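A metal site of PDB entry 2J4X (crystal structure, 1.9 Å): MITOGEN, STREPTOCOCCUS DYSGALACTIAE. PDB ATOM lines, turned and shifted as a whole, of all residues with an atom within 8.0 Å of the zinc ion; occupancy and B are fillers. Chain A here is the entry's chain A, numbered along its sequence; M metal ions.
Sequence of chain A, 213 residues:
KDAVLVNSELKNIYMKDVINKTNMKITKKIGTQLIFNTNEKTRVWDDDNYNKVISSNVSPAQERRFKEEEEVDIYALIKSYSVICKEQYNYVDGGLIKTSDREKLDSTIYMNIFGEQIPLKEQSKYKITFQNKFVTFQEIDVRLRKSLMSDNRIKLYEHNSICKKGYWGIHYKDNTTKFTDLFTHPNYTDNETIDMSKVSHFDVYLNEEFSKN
OG of Ser 200 lies within hydrogen-bond range of ND1 of His 201 (3.1 Å). OD1 of Asp 203 lies close to OD1 of Asn 112, at 3.2 Å. N of Gly 169 is in hydrogen-bond range of O of Asp 203, at 2.7 Å. The backbone NH of Ser 200 lies within hydrogen-bond range of the backbone carbonyl oxygen of His 171. A ring nitrogen (NE2) of His 171 lies within hydrogen-bond range of the side-chain amide oxygen (OD1) of Asn 175, at 3.4 Å.
Three residues have an atom within 4 Å of the zinc ion: His 171, His 201 and Asp 203. The nearest printed residue that does not touch the zinc ion is Tyr 205 (4.9 Å).
The zinc ion is bound by NE2 of His 201 (2.1 Å). OD2 of Asp 203 binds the zinc ion (2.2 Å). ND1 of His 171 is bound to the zinc ion. The zinc ion has three donor atoms within binding distance.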
ATOM      1  N   ASN A 112       8.201  -8.598  -0.704  1.00  0.00           N
ATOM      2  CA  ASN A 112       7.950  -7.397   0.088  1.00  0.00           C
ATOM      3  C   ASN A 112       9.210  -7.141   0.888  1.00  0.00           C
ATOM      4  O   ASN A 112       9.609  -7.994   1.682  1.00  0.00           O
ATOM      5  CB  ASN A 112       6.814  -7.610   1.082  1.00  0.00           C
ATOM      6  CG  ASN A 112       5.512  -7.940   0.403  1.00  0.00           C
ATOM      7  OD1 ASN A 112       4.722  -8.738   0.910  1.00  0.00           O
ATOM      8  ND2 ASN A 112       5.275  -7.322  -0.764  1.00  0.00           N
ATOM      9  N   PHE A 114      11.079  -4.960   3.730  1.00  0.00           N
ATOM     10  CA  PHE A 114      10.842  -4.123   4.904  1.00  0.00           C
ATOM     11  C   PHE A 114      12.134  -3.689   5.529  1.00  0.00           C
ATOM     12  O   PHE A 114      13.087  -4.462   5.571  1.00  0.00           O
ATOM     13  CB  PHE A 114      10.012  -4.880   5.937  1.00  0.00           C
ATOM     14  CG  PHE A 114       8.659  -5.281   5.429  1.00  0.00           C
ATOM     15  CD1 PHE A 114       8.349  -6.619   5.190  1.00  0.00           C
ATOM     16  CD2 PHE A 114       7.698  -4.313   5.157  1.00  0.00           C
ATOM     17  CE1 PHE A 114       7.103  -6.964   4.692  1.00  0.00           C
ATOM     18  CE2 PHE A 114       6.452  -4.659   4.659  1.00  0.00           C
ATOM     19  CZ  PHE A 114       6.151  -5.992   4.420  1.00  0.00           C
ATOM     20  N   GLY A 169      11.188 -14.634   4.463  1.00  0.00           N
ATOM     21  CA  GLY A 169      10.285 -15.758   4.622  1.00  0.00           C
ATOM     22  C   GLY A 169       9.333 -15.982   3.462  1.00  0.00           C
ATOM     23  O   GLY A 169       9.014 -15.084   2.694  1.00  0.00           O
ATOM     24  N   ILE A 170       8.896 -17.228   3.337  1.00  0.00           N
ATOM     25  CA  ILE A 170       7.934 -17.636   2.337  1.00  0.00           C
ATOM     26  C   ILE A 170       6.644 -17.553   3.131  1.00  0.00           C
ATOM     27  O   ILE A 170       6.478 -18.281   4.122  1.00  0.00           O
ATOM     28  CB  ILE A 170       8.170 -19.099   1.909  1.00  0.00           C
ATOM     29  CG1 ILE A 170       9.515 -19.209   1.182  1.00  0.00           C
ATOM     30  CG2 ILE A 170       6.998 -19.591   1.030  1.00  0.00           C
ATOM     31  CD1 ILE A 170       9.987 -20.626   0.964  1.00  0.00           C
ATOM     32  N   HIS A 171       5.756 -16.644   2.741  1.00  0.00           N
ATOM     33  CA  HIS A 171       4.495 -16.501   3.464  1.00  0.00           C
ATOM     34  C   HIS A 171       3.428 -17.254   2.724  1.00  0.00           C
ATOM     35  O   HIS A 171       2.963 -16.840   1.655  1.00  0.00           O
ATOM     36  CB  HIS A 171       4.099 -15.037   3.624  1.00  0.00           C
ATOM     37  CG  HIS A 171       3.214 -14.798   4.813  1.00  0.00           C
ATOM     38  ND1 HIS A 171       3.309 -13.662   5.603  1.00  0.00           N
ATOM     39  CD2 HIS A 171       2.224 -15.546   5.366  1.00  0.00           C
ATOM     40  CE1 HIS A 171       2.416 -13.728   6.582  1.00  0.00           C
ATOM     41  NE2 HIS A 171       1.754 -14.863   6.454  1.00  0.00           N
ATOM     42  N   TYR A 172       3.076 -18.403   3.319  1.00  0.00           N
ATOM     43  CA  TYR A 172       2.085 -19.332   2.799  1.00  0.00           C
ATOM     44  C   TYR A 172       0.671 -18.769   2.871  1.00  0.00           C
ATOM     45  O   TYR A 172       0.400 -17.849   3.658  1.00  0.00           O
ATOM     46  CB  TYR A 172       2.185 -20.662   3.568  1.00  0.00           C
ATOM     47  CG  TYR A 172       3.446 -21.440   3.229  1.00  0.00           C
ATOM     48  CD1 TYR A 172       4.528 -21.467   4.116  1.00  0.00           C
ATOM     49  CD2 TYR A 172       3.585 -22.084   1.993  1.00  0.00           C
ATOM     50  CE1 TYR A 172       5.730 -22.115   3.768  1.00  0.00           C
ATOM     51  CE2 TYR A 172       4.784 -22.726   1.638  1.00  0.00           C
ATOM     52  CZ  TYR A 172       5.849 -22.737   2.533  1.00  0.00           C
ATOM     53  OH  TYR A 172       7.042 -23.336   2.179  1.00  0.00           O
ATOM     54  N   ASN A 175      -1.285 -18.822   6.034  1.00  0.00           N
ATOM     55  CA  ASN A 175      -0.709 -17.941   7.032  1.00  0.00           C
ATOM     56  C   ASN A 175       0.585 -18.426   7.731  1.00  0.00           C
ATOM     57  O   ASN A 175       1.178 -17.690   8.533  1.00  0.00           O
ATOM     58  CB  ASN A 175      -1.773 -17.583   8.076  1.00  0.00           C
ATOM     59  CG  ASN A 175      -1.410 -16.360   8.884  1.00  0.00           C
ATOM     60  OD1 ASN A 175      -1.011 -15.331   8.328  1.00  0.00           O
ATOM     61  ND2 ASN A 175      -1.546 -16.468  10.212  1.00  0.00           N
ATOM     62  N   THR A 176       1.024 -19.649   7.454  1.00  0.00           N
ATOM     63  CA  THR A 176       2.266 -20.120   8.056  1.00  0.00           C
ATOM     64  C   THR A 176       3.429 -19.509   7.267  1.00  0.00           C
ATOM     65  O   THR A 176       3.255 -19.110   6.108  1.00  0.00           O
ATOM     66  CB  THR A 176       2.378 -21.643   8.014  1.00  0.00           C
ATOM     67  OG1 THR A 176       2.297 -22.088   6.657  1.00  0.00           O
ATOM     68  CG2 THR A 176       1.256 -22.276   8.794  1.00  0.00           C
ATOM     69  N   THR A 177       4.605 -19.445   7.883  1.00  0.00           N
ATOM     70  CA  THR A 177       5.791 -18.854   7.241  1.00  0.00           C
ATOM     71  C   THR A 177       7.013 -19.732   7.376  1.00  0.00           C
ATOM     72  O   THR A 177       7.135 -20.493   8.333  1.00  0.00           O
ATOM     73  CB  THR A 177       6.179 -17.511   7.923  1.00  0.00           C
ATOM     74  OG1 THR A 177       5.099 -16.579   7.811  1.00  0.00           O
ATOM     75  CG2 THR A 177       7.419 -16.921   7.272  1.00  0.00           C
ATOM     76  N   PHE A 179      10.935 -19.071   7.573  1.00  0.00           N
ATOM     77  CA  PHE A 179      11.954 -18.027   7.712  1.00  0.00           C
ATOM     78  C   PHE A 179      13.387 -18.515   7.470  1.00  0.00           C
ATOM     79  O   PHE A 179      13.739 -19.651   7.829  1.00  0.00           O
ATOM     80  CB  PHE A 179      11.853 -17.412   9.108  1.00  0.00           C
ATOM     81  CG  PHE A 179      10.638 -16.544   9.327  1.00  0.00           C
ATOM     82  CD1 PHE A 179       9.775 -16.792  10.393  1.00  0.00           C
ATOM     83  CD2 PHE A 179      10.389 -15.442   8.496  1.00  0.00           C
ATOM     84  CE1 PHE A 179       8.675 -15.971  10.634  1.00  0.00           C
ATOM     85  CE2 PHE A 179       9.305 -14.608   8.729  1.00  0.00           C
ATOM     86  CZ  PHE A 179       8.440 -14.880   9.802  1.00  0.00           C
ATOM     87  N   SER A 200       1.876 -17.507  -0.824  1.00  0.00           N
ATOM     88  CA  SER A 200       1.195 -16.265  -1.116  1.00  0.00           C
ATOM     89  C   SER A 200       2.238 -15.258  -1.595  1.00  0.00           C
ATOM     90  O   SER A 200       2.148 -14.766  -2.728  1.00  0.00           O
ATOM     91  CB  SER A 200       0.478 -15.735   0.100  1.00  0.00           C
ATOM     92  OG  SER A 200      -0.137 -14.497  -0.210  1.00  0.00           O
ATOM     93  N   HIS A 201       3.238 -14.965  -0.769  1.00  0.00           N
ATOM     94  CA  HIS A 201       4.272 -14.010  -1.149  1.00  0.00           C
ATOM     95  C   HIS A 201       5.553 -14.230  -0.374  1.00  0.00           C
ATOM     96  O   HIS A 201       5.611 -15.139   0.462  1.00  0.00           O
ATOM     97  CB  HIS A 201       3.806 -12.577  -0.889  1.00  0.00           C
ATOM     98  CG  HIS A 201       3.353 -12.354   0.516  1.00  0.00           C
ATOM     99  ND1 HIS A 201       2.119 -12.753   0.986  1.00  0.00           N
ATOM    100  CD2 HIS A 201       3.980 -11.766   1.569  1.00  0.00           C
ATOM    101  CE1 HIS A 201       1.995 -12.422   2.258  1.00  0.00           C
ATOM    102  NE2 HIS A 201       3.107 -11.821   2.640  1.00  0.00           N
ATOM    103  N   PHE A 202       6.572 -13.420  -0.657  1.00  0.00           N
ATOM    104  CA  PHE A 202       7.852 -13.508   0.043  1.00  0.00           C
ATOM    105  C   PHE A 202       8.039 -12.216   0.846  1.00  0.00           C
ATOM    106  O   PHE A 202       7.733 -11.133   0.342  1.00  0.00           O
ATOM    107  CB  PHE A 202       9.025 -13.638  -0.938  1.00  0.00           C
ATOM    108  CG  PHE A 202       8.982 -14.889  -1.775  1.00  0.00           C
ATOM    109  CD1 PHE A 202       9.403 -14.854  -3.102  1.00  0.00           C
ATOM    110  CD2 PHE A 202       8.494 -16.080  -1.253  1.00  0.00           C
ATOM    111  CE1 PHE A 202       9.334 -16.003  -3.900  1.00  0.00           C
ATOM    112  CE2 PHE A 202       8.415 -17.233  -2.037  1.00  0.00           C
ATOM    113  CZ  PHE A 202       8.843 -17.187  -3.371  1.00  0.00           C
ATOM    114  N   ASP A 203       8.518 -12.343   2.090  1.00  0.00           N
ATOM    115  CA  ASP A 203       8.763 -11.197   2.958  1.00  0.00           C
ATOM    116  C   ASP A 203      10.236 -11.063   3.314  1.00  0.00           C
ATOM    117  O   ASP A 203      10.843 -12.015   3.793  1.00  0.00           O
ATOM    118  CB  ASP A 203       7.970 -11.298   4.258  1.00  0.00           C
ATOM    119  CG  ASP A 203       6.486 -11.056   4.058  1.00  0.00           C
ATOM    120  OD1 ASP A 203       6.109 -10.019   3.436  1.00  0.00           O
ATOM    121  OD2 ASP A 203       5.701 -11.896   4.536  1.00  0.00           O
ATOM    122  N   VAL A 204      10.794  -9.887   3.087  1.00  0.00           N
ATOM    123  CA  VAL A 204      12.202  -9.646   3.384  1.00  0.00           C
ATOM    124  C   VAL A 204      12.295  -8.691   4.567  1.00  0.00           C
ATOM    125  O   VAL A 204      11.719  -7.615   4.521  1.00  0.00           O
ATOM    126  CB  VAL A 204      12.900  -9.039   2.169  1.00  0.00           C
ATOM    127  CG1 VAL A 204      14.369  -8.873   2.442  1.00  0.00           C
ATOM    128  CG2 VAL A 204      12.666  -9.911   0.952  1.00  0.00           C
ATOM    129  N   TYR A 205      13.008  -9.078   5.633  1.00  0.00           N
ATOM    130  CA  TYR A 205      13.147  -8.242   6.825  1.00  0.00           C
ATOM    131  C   TYR A 205      14.548  -7.737   7.050  1.00  0.00           C
ATOM    132  O   TYR A 205      15.331  -8.372   7.754  1.00  0.00           O
ATOM    133  CB  TYR A 205      12.702  -9.004   8.076  1.00  0.00           C
ATOM    134  CG  TYR A 205      11.265  -9.399   8.003  1.00  0.00           C
ATOM    135  CD1 TYR A 205      10.878 -10.643   7.493  1.00  0.00           C
ATOM    136  CD2 TYR A 205      10.277  -8.495   8.354  1.00  0.00           C
ATOM    137  CE1 TYR A 205       9.533 -10.978   7.353  1.00  0.00           C
ATOM    138  CE2 TYR A 205       8.934  -8.807   8.208  1.00  0.00           C
ATOM    139  CZ  TYR A 205       8.575 -10.040   7.711  1.00  0.00           C
ATOM    140  OH  TYR A 205       7.232 -10.323   7.594  1.00  0.00           O
HETATM  141 ZN    ZN M   1       3.535 -11.656   4.691  1.00  0.00          ZN
